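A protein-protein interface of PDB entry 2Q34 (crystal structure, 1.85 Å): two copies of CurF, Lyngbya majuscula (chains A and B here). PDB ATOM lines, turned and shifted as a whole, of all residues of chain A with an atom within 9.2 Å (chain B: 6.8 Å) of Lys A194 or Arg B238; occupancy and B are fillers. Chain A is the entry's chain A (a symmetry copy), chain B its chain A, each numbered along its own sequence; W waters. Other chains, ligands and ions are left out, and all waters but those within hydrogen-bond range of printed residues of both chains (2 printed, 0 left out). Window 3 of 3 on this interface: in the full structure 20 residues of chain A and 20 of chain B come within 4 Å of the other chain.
The side-chain hydroxyl of Thr B157 sits close to the backbone NH of Glu B159. The side-chain amino group (NZ) of Lys A49 lies within hydrogen-bond range of the backbone carbonyl oxygen (O) of Ser A195 (2.8 Å).
Among the printed residues, pairs that only touch across the chains: Ser A195 with Arg B238 (3.9 Å), Pro A196 with Gly B131 (3.4 Å), Pro A196 with Glu B234 (3.7 Å), Pro A196 with Arg B238 (3.8 Å), Ser A199 with Met B128 (3.9 Å), Ser A199 with Phe B132 (3.96 Å) and Leu A200 with Met B128 (3.7 Å).
Water W2 bridges O of Met B128 (2.8 Å) and OG of Ser A195 (2.9 Å). Water W1 lies within hydrogen-bond range of O of Lys A191 (2.8 Å) and O of Thr B157 (2.9 Å).
Of the 17 printed residues of chain B, 6 touch a printed residue of chain A. Printed residues of chain B that touch a printed residue of chain A: Met B128, Gly B131, Phe B132, Glu B159, Glu B234 and Arg B238. Hydrophobic or aromatic side chains of chain B that line the printed part of chain A: Met B128. Among the printed residues, Asp or Glu carboxylates within 4 Å of a Lys or Arg side-chain nitrogen of the other chain: Lys A191 with Glu B159 (3.7 Å).
Asn A11 touches none of the printed residues of chain B. Of chain B, only Arg B238 (2.4 Å) comes within 4 Å of Lys A194. Of the printed residues of chain B, Ser A195 touches Met B128 and Arg B238. Arg A197 touches none of the printed residues of chain B. Of the printed residues of chain B, Ser A199 touches Met B128, Gly B131 and Phe B132. Of the printed residues of chain A, Glu B159 touches Lys A191 (3.7 Å). No residue of chain A comes within 4 Å of Ser B237. Arg B238 touches three residues of chain A. The nearest residue of chain B that does not touch Lys A194 is Glu B159 (5.4 Å). The nearest residue of chain A that does not touch Arg B238 is Lys A49 (5.0 Å). The nearest printed residue of chain A that does not touch Met B128 is Pro A196 (5.2 Å).
The side-chain hydroxyl of Ser A195 is in hydrogen-bond range of the backbone carbonyl oxygen of Met B128 (3.3 Å). OG of Ser A199 lies within hydrogen-bond range of O of Gly B131. OE1 of Glu B159 lies within salt-bridge range of NZ of Lys A191, 3.7 Å away. The guanidinium group (NH2) of Arg B238 lies within hydrogen-bond range of the backbone carbonyl oxygen (O) of Lys A194 (2.4 Å).
No position is printed for both chains. Of the 11 pairs that touch across the chains among the printed residues, none has its exchanged pair printed and touching as well.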
ATOM      1  N   GLY A  10      18.437   8.512 -19.766  1.00  0.00           N
ATOM      2  CA  GLY A  10      17.591   9.115 -18.721  1.00  0.00           C
ATOM      3  C   GLY A  10      18.220  10.333 -18.060  1.00  0.00           C
ATOM      4  O   GLY A  10      19.445  10.422 -17.935  1.00  0.00           O
ATOM      5  N   ASN A  11      17.374  11.285 -17.671  1.00  0.00           N
ATOM      6  CA  ASN A  11      17.817  12.498 -16.953  1.00  0.00           C
ATOM      7  C   ASN A  11      18.779  13.396 -17.726  1.00  0.00           C
ATOM      8  O   ASN A  11      19.495  14.220 -17.124  1.00  0.00           O
ATOM      9  CB  ASN A  11      18.434  12.133 -15.607  1.00  0.00           C
ATOM     10  CG  ASN A  11      17.536  11.249 -14.792  1.00  0.00           C
ATOM     11  OD1 ASN A  11      16.368  11.566 -14.587  1.00  0.00           O
ATOM     12  ND2 ASN A  11      18.069  10.121 -14.341  1.00  0.00           N
ATOM     13  N   GLY A  12      18.742  13.277 -19.053  1.00  0.00           N
ATOM     14  CA  GLY A  12      19.580  14.088 -19.919  1.00  0.00           C
ATOM     15  C   GLY A  12      20.949  13.500 -20.206  1.00  0.00           C
ATOM     16  O   GLY A  12      21.753  14.158 -20.873  1.00  0.00           O
ATOM     17  N   VAL A  13      21.218  12.292 -19.701  1.00  0.00           N
ATOM     18  CA  VAL A  13      22.492  11.562 -19.997  1.00  0.00           C
ATOM     19  C   VAL A  13      22.275  10.769 -21.307  1.00  0.00           C
ATOM     20  O   VAL A  13      21.285  10.040 -21.445  1.00  0.00           O
ATOM     21  CB  VAL A  13      22.936  10.651 -18.829  1.00  0.00           C
ATOM     22  CG1 VAL A  13      24.237   9.932 -19.143  1.00  0.00           C
ATOM     23  CG2 VAL A  13      23.099  11.467 -17.545  1.00  0.00           C
ATOM     24  N   LYS A  49      22.250  16.773 -21.300  1.00  0.00           N
ATOM     25  CA  LYS A  49      23.115  17.448 -20.346  1.00  0.00           C
ATOM     26  C   LYS A  49      24.519  16.830 -20.232  1.00  0.00           C
ATOM     27  O   LYS A  49      25.451  17.501 -19.763  1.00  0.00           O
ATOM     28  CB  LYS A  49      22.504  17.356 -18.949  1.00  0.00           C
ATOM     29  CG  LYS A  49      21.211  18.146 -18.743  1.00  0.00           C
ATOM     30  CD  LYS A  49      20.864  17.988 -17.266  1.00  0.00           C
ATOM     31  CE  LYS A  49      19.678  18.801 -16.879  1.00  0.00           C
ATOM     32  NZ  LYS A  49      19.460  18.593 -15.434  1.00  0.00           N
ATOM     33  N   VAL A  50      24.637  15.533 -20.538  1.00  0.00           N
ATOM     34  CA  VAL A  50      25.930  14.828 -20.463  1.00  0.00           C
ATOM     35  C   VAL A  50      25.993  13.773 -21.544  1.00  0.00           C
ATOM     36  O   VAL A  50      25.031  13.018 -21.754  1.00  0.00           O
ATOM     37  CB  VAL A  50      26.104  14.067 -19.131  1.00  0.00           C
ATOM     38  CG1 VAL A  50      27.502  13.420 -19.032  1.00  0.00           C
ATOM     39  CG2 VAL A  50      25.834  14.965 -17.902  1.00  0.00           C
ATOM     40  N   GLN A 187      27.235   6.173 -14.061  1.00  0.00           N
ATOM     41  CA  GLN A 187      26.948   6.679 -12.704  1.00  0.00           C
ATOM     42  C   GLN A 187      27.473   8.088 -12.497  1.00  0.00           C
ATOM     43  O   GLN A 187      26.807   8.921 -11.869  1.00  0.00           O
ATOM     44  CB  GLN A 187      27.530   5.759 -11.647  1.00  0.00           C
ATOM     45  CG  GLN A 187      26.721   4.468 -11.505  1.00  0.00           C
ATOM     46  CD  GLN A 187      27.347   3.472 -10.547  1.00  0.00           C
ATOM     47  OE1 GLN A 187      27.718   3.818  -9.414  1.00  0.00           O
ATOM     48  NE2 GLN A 187      27.446   2.216 -10.987  1.00  0.00           N
ATOM     49  N   LEU A 188      28.671   8.349 -13.004  1.00  0.00           N
ATOM     50  CA  LEU A 188      29.228   9.699 -12.947  1.00  0.00           C
ATOM     51  C   LEU A 188      28.353  10.682 -13.756  1.00  0.00           C
ATOM     52  O   LEU A 188      28.099  11.808 -13.311  1.00  0.00           O
ATOM     53  CB  LEU A 188      30.680   9.684 -13.452  1.00  0.00           C
ATOM     54  CG  LEU A 188      31.368  11.045 -13.577  1.00  0.00           C
ATOM     55  CD1 LEU A 188      31.411  11.790 -12.219  1.00  0.00           C
ATOM     56  CD2 LEU A 188      32.760  10.889 -14.217  1.00  0.00           C
ATOM     57  N   GLY A 189      27.889  10.258 -14.935  1.00  0.00           N
ATOM     58  CA  GLY A 189      27.071  11.124 -15.796  1.00  0.00           C
ATOM     59  C   GLY A 189      25.804  11.513 -15.063  1.00  0.00           C
ATOM     60  O   GLY A 189      25.389  12.670 -15.086  1.00  0.00           O
ATOM     61  N   GLN A 190      25.187  10.540 -14.410  1.00  0.00           N
ATOM     62  CA  GLN A 190      23.955  10.801 -13.629  1.00  0.00           C
ATOM     63  C   GLN A 190      24.176  11.801 -12.496  1.00  0.00           C
ATOM     64  O   GLN A 190      23.330  12.664 -12.261  1.00  0.00           O
ATOM     65  CB  GLN A 190      23.315   9.509 -13.123  1.00  0.00           C
ATOM     66  CG  GLN A 190      22.781   8.566 -14.234  1.00  0.00           C
ATOM     67  CD  GLN A 190      21.604   9.161 -15.043  1.00  0.00           C
ATOM     68  OE1 GLN A 190      20.891  10.028 -14.576  1.00  0.00           O
ATOM     69  NE2 GLN A 190      21.411   8.666 -16.254  1.00  0.00           N
ATOM     70  N   LYS A 191      25.325  11.716 -11.821  1.00  0.00           N
ATOM     71  CA  LYS A 191      25.669  12.727 -10.790  1.00  0.00           C
ATOM     72  C   LYS A 191      25.770  14.116 -11.387  1.00  0.00           C
ATOM     73  O   LYS A 191      25.230  15.088 -10.845  1.00  0.00           O
ATOM     74  CB  LYS A 191      26.997  12.396 -10.103  1.00  0.00           C
ATOM     75  CG  LYS A 191      26.921  11.228  -9.163  1.00  0.00           C
ATOM     76  CD  LYS A 191      28.283  10.899  -8.589  1.00  0.00           C
ATOM     77  CE  LYS A 191      28.172   9.732  -7.626  1.00  0.00           C
ATOM     78  NZ  LYS A 191      29.529   9.302  -7.189  1.00  0.00           N
ATOM     79  N   ILE A 192      26.477  14.224 -12.504  1.00  0.00           N
ATOM     80  CA  ILE A 192      26.655  15.521 -13.163  1.00  0.00           C
ATOM     81  C   ILE A 192      25.325  16.093 -13.661  1.00  0.00           C
ATOM     82  O   ILE A 192      25.048  17.294 -13.487  1.00  0.00           O
ATOM     83  CB  ILE A 192      27.688  15.398 -14.313  1.00  0.00           C
ATOM     84  CG1 ILE A 192      29.060  15.057 -13.713  1.00  0.00           C
ATOM     85  CG2 ILE A 192      27.771  16.692 -15.136  1.00  0.00           C
ATOM     86  CD1 ILE A 192      30.068  14.551 -14.758  1.00  0.00           C
ATOM     87  N   ALA A 193      24.475  15.224 -14.209  1.00  0.00           N
ATOM     88  CA  ALA A 193      23.180  15.628 -14.773  1.00  0.00           C
ATOM     89  C   ALA A 193      22.169  16.164 -13.741  1.00  0.00           C
ATOM     90  O   ALA A 193      21.082  16.630 -14.110  1.00  0.00           O
ATOM     91  CB  ALA A 193      22.565  14.472 -15.542  1.00  0.00           C
ATOM     92  N   LYS A 194      22.518  16.103 -12.460  1.00  0.00           N
ATOM     93  CA  LYS A 194      21.649  16.696 -11.428  1.00  0.00           C
ATOM     94  C   LYS A 194      21.591  18.225 -11.508  1.00  0.00           C
ATOM     95  O   LYS A 194      20.639  18.838 -11.018  1.00  0.00           O
ATOM     96  CB  LYS A 194      22.073  16.239 -10.034  1.00  0.00           C
ATOM     97  CG  LYS A 194      21.761  14.747  -9.804  1.00  0.00           C
ATOM     98  CD  LYS A 194      22.034  14.298  -8.391  1.00  0.00           C
ATOM     99  CE  LYS A 194      21.507  12.883  -8.187  1.00  0.00           C
ATOM    100  NZ  LYS A 194      21.574  12.458  -6.757  1.00  0.00           N
ATOM    101  N   SER A 195      22.629  18.837 -12.073  1.00  0.00           N
ATOM    102  CA  SER A 195      22.681  20.294 -12.225  1.00  0.00           C
ATOM    103  C   SER A 195      21.856  20.784 -13.400  1.00  0.00           C
ATOM    104  O   SER A 195      21.641  20.033 -14.371  1.00  0.00           O
ATOM    105  CB  SER A 195      24.138  20.746 -12.379  1.00  0.00           C
ATOM    106  OG  SER A 195      24.831  20.465 -11.176  1.00  0.00           O
ATOM    107  N   PRO A 196      21.407  22.054 -13.346  1.00  0.00           N
ATOM    108  CA  PRO A 196      20.696  22.634 -14.477  1.00  0.00           C
ATOM    109  C   PRO A 196      21.621  22.694 -15.678  1.00  0.00           C
ATOM    110  O   PRO A 196      22.816  22.943 -15.534  1.00  0.00           O
ATOM    111  CB  PRO A 196      20.381  24.074 -14.003  1.00  0.00           C
ATOM    112  CG  PRO A 196      20.535  24.044 -12.521  1.00  0.00           C
ATOM    113  CD  PRO A 196      21.571  23.025 -12.244  1.00  0.00           C
ATOM    114  N   ARG A 197      21.067  22.490 -16.863  1.00  0.00           N
ATOM    115  CA  ARG A 197      21.857  22.547 -18.072  1.00  0.00           C
ATOM    116  C   ARG A 197      22.601  23.874 -18.251  1.00  0.00           C
ATOM    117  O   ARG A 197      23.760  23.897 -18.697  1.00  0.00           O
ATOM    118  CB  ARG A 197      20.958  22.307 -19.275  1.00  0.00           C
ATOM    119  CG  ARG A 197      21.752  22.009 -20.528  1.00  0.00           C
ATOM    120  CD  ARG A 197      20.847  21.763 -21.719  1.00  0.00           C
ATOM    121  NE  ARG A 197      21.616  21.403 -22.916  1.00  0.00           N
ATOM    122  CZ  ARG A 197      22.192  22.288 -23.722  1.00  0.00           C
ATOM    123  NH1 ARG A 197      22.099  23.578 -23.455  1.00  0.00           N
ATOM    124  NH2 ARG A 197      22.872  21.892 -24.790  1.00  0.00           N
ATOM    125  N   LEU A 198      21.938  24.985 -17.931  1.00  0.00           N
ATOM    126  CA  LEU A 198      22.556  26.291 -18.118  1.00  0.00           C
ATOM    127  C   LEU A 198      23.853  26.362 -17.313  1.00  0.00           C
ATOM    128  O   LEU A 198      24.868  26.872 -17.792  1.00  0.00           O
ATOM    129  CB  LEU A 198      21.602  27.417 -17.689  1.00  0.00           C
ATOM    130  CG  LEU A 198      22.013  28.834 -18.129  1.00  0.00           C
ATOM    131  CD1 LEU A 198      21.608  29.124 -19.565  1.00  0.00           C
ATOM    132  CD2 LEU A 198      21.410  29.880 -17.212  1.00  0.00           C
ATOM    133  N   SER A 199      23.811  25.831 -16.096  1.00  0.00           N
ATOM    134  CA  SER A 199      24.956  25.871 -15.215  1.00  0.00           C
ATOM    135  C   SER A 199      26.077  24.960 -15.739  1.00  0.00           C
ATOM    136  O   SER A 199      27.247  25.341 -15.718  1.00  0.00           O
ATOM    137  CB  SER A 199      24.540  25.482 -13.801  1.00  0.00           C
ATOM    138  OG  SER A 199      23.648  26.473 -13.285  1.00  0.00           O
ATOM    139  N   LEU A 200      25.714  23.766 -16.203  1.00  0.00           N
ATOM    140  CA  LEU A 200      26.706  22.850 -16.786  1.00  0.00           C
ATOM    141  C   LEU A 200      27.429  23.497 -17.975  1.00  0.00           C
ATOM    142  O   LEU A 200      28.661  23.395 -18.103  1.00  0.00           O
ATOM    143  CB  LEU A 200      26.047  21.519 -17.202  1.00  0.00           C
ATOM    144  CG  LEU A 200      25.548  20.588 -16.089  1.00  0.00           C
ATOM    145  CD1 LEU A 200      24.830  19.402 -16.765  1.00  0.00           C
ATOM    146  CD2 LEU A 200      26.773  20.105 -15.267  1.00  0.00           C
ATOM    147  N   MET B 128      27.467  23.693  -7.055  1.00  0.00           N
ATOM    148  CA  MET B 128      26.681  23.011  -8.082  1.00  0.00           C
ATOM    149  C   MET B 128      25.582  22.112  -7.523  1.00  0.00           C
ATOM    150  O   MET B 128      24.618  21.814  -8.221  1.00  0.00           O
ATOM    151  CB  MET B 128      27.578  22.277  -9.073  1.00  0.00           C
ATOM    152  CG  MET B 128      28.339  23.254  -9.972  1.00  0.00           C
ATOM    153  SD  MET B 128      27.211  24.129 -11.287  1.00  0.00           S
ATOM    154  CE  MET B 128      27.220  22.685 -12.649  1.00  0.00           C
ATOM    155  N   LYS B 129      25.704  21.717  -6.264  1.00  0.00           N
ATOM    156  CA  LYS B 129      24.618  20.995  -5.600  1.00  0.00           C
ATOM    157  C   LYS B 129      23.343  21.853  -5.536  1.00  0.00           C
ATOM    158  O   LYS B 129      22.237  21.368  -5.801  1.00  0.00           O
ATOM    159  CB  LYS B 129      25.065  20.523  -4.207  1.00  0.00           C
ATOM    160  CG  LYS B 129      23.968  19.834  -3.374  1.00  0.00           C
ATOM    161  CD  LYS B 129      24.562  18.887  -2.327  1.00  0.00           C
ATOM    162  CE  LYS B 129      24.608  17.421  -2.826  1.00  0.00           C
ATOM    163  NZ  LYS B 129      25.408  16.476  -1.945  1.00  0.00           N
ATOM    164  N   TYR B 130      23.500  23.132  -5.200  1.00  0.00           N
ATOM    165  CA  TYR B 130      22.396  24.075  -5.237  1.00  0.00           C
ATOM    166  C   TYR B 130      22.026  24.465  -6.656  1.00  0.00           C
ATOM    167  O   TYR B 130      20.961  25.039  -6.875  1.00  0.00           O
ATOM    168  CB  TYR B 130      22.742  25.351  -4.485  1.00  0.00           C
ATOM    169  CG  TYR B 130      23.176  25.142  -3.062  1.00  0.00           C
ATOM    170  CD1 TYR B 130      22.250  24.843  -2.072  1.00  0.00           C
ATOM    171  CD2 TYR B 130      24.506  25.283  -2.704  1.00  0.00           C
ATOM    172  CE1 TYR B 130      22.647  24.662  -0.759  1.00  0.00           C
ATOM    173  CE2 TYR B 130      24.917  25.115  -1.388  1.00  0.00           C
ATOM    174  CZ  TYR B 130      23.982  24.796  -0.429  1.00  0.00           C
ATOM    175  OH  TYR B 130      24.377  24.635   0.880  1.00  0.00           O
ATOM    176  N   GLY B 131      22.931  24.212  -7.599  1.00  0.00           N
ATOM    177  CA  GLY B 131      22.614  24.366  -9.017  1.00  0.00           C
ATOM    178  C   GLY B 131      23.265  25.556  -9.713  1.00  0.00           C
ATOM    179  O   GLY B 131      22.908  25.873 -10.844  1.00  0.00           O
ATOM    180  N   PHE B 132      24.211  26.213  -9.043  1.00  0.00           N
ATOM    181  CA  PHE B 132      24.879  27.377  -9.626  1.00  0.00           C
ATOM    182  C   PHE B 132      26.393  27.239  -9.537  1.00  0.00           C
ATOM    183  O   PHE B 132      26.917  26.383  -8.829  1.00  0.00           O
ATOM    184  CB  PHE B 132      24.405  28.702  -8.995  1.00  0.00           C
ATOM    185  CG  PHE B 132      24.471  28.717  -7.483  1.00  0.00           C
ATOM    186  CD1 PHE B 132      25.674  28.869  -6.827  1.00  0.00           C
ATOM    187  CD2 PHE B 132      23.303  28.586  -6.731  1.00  0.00           C
ATOM    188  CE1 PHE B 132      25.733  28.865  -5.411  1.00  0.00           C
ATOM    189  CE2 PHE B 132      23.359  28.605  -5.328  1.00  0.00           C
ATOM    190  CZ  PHE B 132      24.552  28.733  -4.695  1.00  0.00           C
ATOM    191  N   THR B 157      30.099  17.972  -9.733  1.00  0.00           N
ATOM    192  CA  THR B 157      29.137  17.199  -8.932  1.00  0.00           C
ATOM    193  C   THR B 157      28.625  17.953  -7.693  1.00  0.00           C
ATOM    194  O   THR B 157      27.480  17.762  -7.281  1.00  0.00           O
ATOM    195  CB  THR B 157      29.674  15.809  -8.488  1.00  0.00           C
ATOM    196  OG1 THR B 157      30.647  15.960  -7.448  1.00  0.00           O
ATOM    197  CG2 THR B 157      30.267  15.028  -9.633  1.00  0.00           C
ATOM    198  N   GLU B 159      29.476  17.243  -4.836  1.00  0.00           N
ATOM    199  CA  GLU B 159      29.287  16.194  -3.831  1.00  0.00           C
ATOM    200  C   GLU B 159      30.241  16.289  -2.639  1.00  0.00           C
ATOM    201  O   GLU B 159      31.297  16.939  -2.711  1.00  0.00           O
ATOM    202  CB  GLU B 159      29.431  14.791  -4.458  1.00  0.00           C
ATOM    203  CG  GLU B 159      28.216  14.342  -5.232  1.00  0.00           C
ATOM    204  CD  GLU B 159      27.938  12.859  -5.069  1.00  0.00           C
ATOM    205  OE1 GLU B 159      28.902  12.078  -4.890  1.00  0.00           O
ATOM    206  OE2 GLU B 159      26.745  12.482  -5.116  1.00  0.00           O
ATOM    207  N   GLU B 234      14.688  28.171 -11.121  1.00  0.00           N
ATOM    208  CA  GLU B 234      14.637  26.970 -10.285  1.00  0.00           C
ATOM    209  C   GLU B 234      15.597  26.960  -9.089  1.00  0.00           C
ATOM    210  O   GLU B 234      15.522  26.070  -8.242  1.00  0.00           O
ATOM    211  CB  GLU B 234      14.884  25.733 -11.154  1.00  0.00           C
ATOM    212  CG  GLU B 234      16.294  25.659 -11.764  1.00  0.00           C
ATOM    213  CD  GLU B 234      16.372  26.220 -13.178  1.00  0.00           C
ATOM    214  OE1 GLU B 234      16.944  25.525 -14.044  1.00  0.00           O
ATOM    215  OE2 GLU B 234      15.867  27.339 -13.433  1.00  0.00           O
ATOM    216  N   ILE B 235      16.493  27.941  -9.009  1.00  0.00           N
ATOM    217  CA  ILE B 235      17.502  27.963  -7.946  1.00  0.00           C
ATOM    218  C   ILE B 235      16.932  28.092  -6.537  1.00  0.00           C
ATOM    219  O   ILE B 235      17.403  27.426  -5.624  1.00  0.00           O
ATOM    220  CB  ILE B 235      18.570  29.057  -8.177  1.00  0.00           C
ATOM    221  CG1 ILE B 235      19.284  28.828  -9.524  1.00  0.00           C
ATOM    222  CG2 ILE B 235      19.566  29.108  -7.006  1.00  0.00           C
ATOM    223  CD1 ILE B 235      19.970  27.455  -9.671  1.00  0.00           C
ATOM    224  N   ALA B 236      15.927  28.943  -6.357  1.00  0.00           N
ATOM    225  CA  ALA B 236      15.351  29.158  -5.015  1.00  0.00           C
ATOM    226  C   ALA B 236      14.842  27.848  -4.416  1.00  0.00           C
ATOM    227  O   ALA B 236      15.118  27.526  -3.246  1.00  0.00           O
ATOM    228  CB  ALA B 236      14.253  30.191  -5.068  1.00  0.00           C
ATOM    229  N   SER B 237      14.135  27.089  -5.244  1.00  0.00           N
ATOM    230  CA  SER B 237      13.585  25.800  -4.849  1.00  0.00           C
ATOM    231  C   SER B 237      14.663  24.768  -4.559  1.00  0.00           C
ATOM    232  O   SER B 237      14.506  23.947  -3.656  1.00  0.00           O
ATOM    233  CB  SER B 237      12.641  25.285  -5.934  1.00  0.00           C
ATOM    234  OG  SER B 237      12.248  23.954  -5.658  1.00  0.00           O
ATOM    235  N   ARG B 238      15.750  24.785  -5.342  1.00  0.00           N
ATOM    236  CA  ARG B 238      16.882  23.881  -5.112  1.00  0.00           C
ATOM    237  C   ARG B 238      17.538  24.168  -3.781  1.00  0.00           C
ATOM    238  O   ARG B 238      17.917  23.239  -3.054  1.00  0.00           O
ATOM    239  CB  ARG B 238      17.925  24.006  -6.236  1.00  0.00           C
ATOM    240  CG  ARG B 238      17.601  23.145  -7.438  1.00  0.00           C
ATOM    241  CD  ARG B 238      18.573  23.423  -8.568  1.00  0.00           C
ATOM    242  NE  ARG B 238      18.406  22.448  -9.636  1.00  0.00           N
ATOM    243  CZ  ARG B 238      19.198  21.394  -9.829  1.00  0.00           C
ATOM    244  NH1 ARG B 238      20.242  21.172  -9.042  1.00  0.00           N
ATOM    245  NH2 ARG B 238      18.950  20.582 -10.834  1.00  0.00           N
ATOM    246  N   ILE B 239      17.654  25.454  -3.451  1.00  0.00           N
ATOM    247  CA  ILE B 239      18.237  25.862  -2.171  1.00  0.00           C
ATOM    248  C   ILE B 239      17.312  25.424  -1.031  1.00  0.00           C
ATOM    249  O   ILE B 239      17.780  24.899  -0.032  1.00  0.00           O
ATOM    250  CB  ILE B 239      18.540  27.381  -2.099  1.00  0.00           C
ATOM    251  CG1 ILE B 239      19.595  27.769  -3.155  1.00  0.00           C
ATOM    252  CG2 ILE B 239      19.053  27.769  -0.705  1.00  0.00           C
ATOM    253  CD1 ILE B 239      19.708  29.260  -3.366  1.00  0.00           C
ATOM    254  N   GLN B 240      16.012  25.607  -1.213  1.00  0.00           N
ATOM    255  CA  GLN B 240      15.016  25.170  -0.203  1.00  0.00           C
ATOM    256  C   GLN B 240      15.181  23.703   0.138  1.00  0.00           C
ATOM    257  O   GLN B 240      15.089  23.317   1.307  1.00  0.00           O
ATOM    258  CB  GLN B 240      13.585  25.402  -0.694  1.00  0.00           C
ATOM    259  CG  GLN B 240      12.507  24.920   0.281  1.00  0.00           C
ATOM    260  CD  GLN B 240      11.122  25.422  -0.074  1.00  0.00           C
ATOM    261  OE1 GLN B 240      10.958  26.559  -0.520  1.00  0.00           O
ATOM    262  NE2 GLN B 240      10.115  24.584   0.137  1.00  0.00           N
ATOM    263  N   GLN B 241      15.422  22.879  -0.882  1.00  0.00           N
ATOM    264  CA  GLN B 241      15.500  21.436  -0.649  1.00  0.00           C
ATOM    265  C   GLN B 241      16.822  20.944  -0.054  1.00  0.00           C
ATOM    266  O   GLN B 241      16.906  19.802   0.389  1.00  0.00           O
ATOM    267  CB  GLN B 241      15.090  20.660  -1.899  1.00  0.00           C
ATOM    268  CG  GLN B 241      13.662  20.966  -2.334  1.00  0.00           C
ATOM    269  CD  GLN B 241      12.629  20.752  -1.216  1.00  0.00           C
ATOM    270  OE1 GLN B 241      11.699  21.542  -1.061  1.00  0.00           O
ATOM    271  NE2 GLN B 241      12.798  19.688  -0.439  1.00  0.00           N
ATOM    272  N   GLU B 242      17.830  21.821   0.001  1.00  0.00           N
ATOM    273  CA  GLU B 242      19.106  21.486   0.644  1.00  0.00           C
ATOM    274  C   GLU B 242      19.143  21.762   2.149  1.00  0.00           C
ATOM    275  O   GLU B 242      20.042  21.280   2.842  1.00  0.00           O
ATOM    276  CB  GLU B 242      20.268  22.166  -0.062  1.00  0.00           C
ATOM    277  CG  GLU B 242      20.509  21.683  -1.503  1.00  0.00           C
ATOM    278  CD  GLU B 242      20.847  20.199  -1.600  1.00  0.00           C
ATOM    279  OE1 GLU B 242      21.696  19.709  -0.822  1.00  0.00           O
ATOM    280  OE2 GLU B 242      20.266  19.518  -2.470  1.00  0.00           O
ATOM    281  N   PHE B 243      18.175  22.533   2.658  1.00  0.00           N
ATOM    282  CA  PHE B 243      17.917  22.621   4.107  1.00  0.00           C
ATOM    283  C   PHE B 243      17.712  21.255   4.772  1.00  0.00           C
ATOM    284  O   PHE B 243      17.314  20.282   4.117  1.00  0.00           O
ATOM    285  CB  PHE B 243      16.664  23.458   4.375  1.00  0.00           C
ATOM    286  CG  PHE B 243      16.941  24.894   4.659  1.00  0.00           C
ATOM    287  CD1 PHE B 243      16.932  25.364   5.967  1.00  0.00           C
ATOM    288  CD2 PHE B 243      17.204  25.783   3.619  1.00  0.00           C
ATOM    289  CE1 PHE B 243      17.188  26.702   6.245  1.00  0.00           C
ATOM    290  CE2 PHE B 243      17.459  27.132   3.880  1.00  0.00           C
ATOM    291  CZ  PHE B 243      17.449  27.593   5.208  1.00  0.00           C
ATOM    292  OXT PHE B 243      17.899  21.092   5.991  1.00  0.00           O
HETATM  293  O   HOH W   1      25.688  15.644  -8.119  1.00  0.00           O
HETATM  294  O   HOH W   2      23.613  19.300  -8.856  1.00  0.00           O
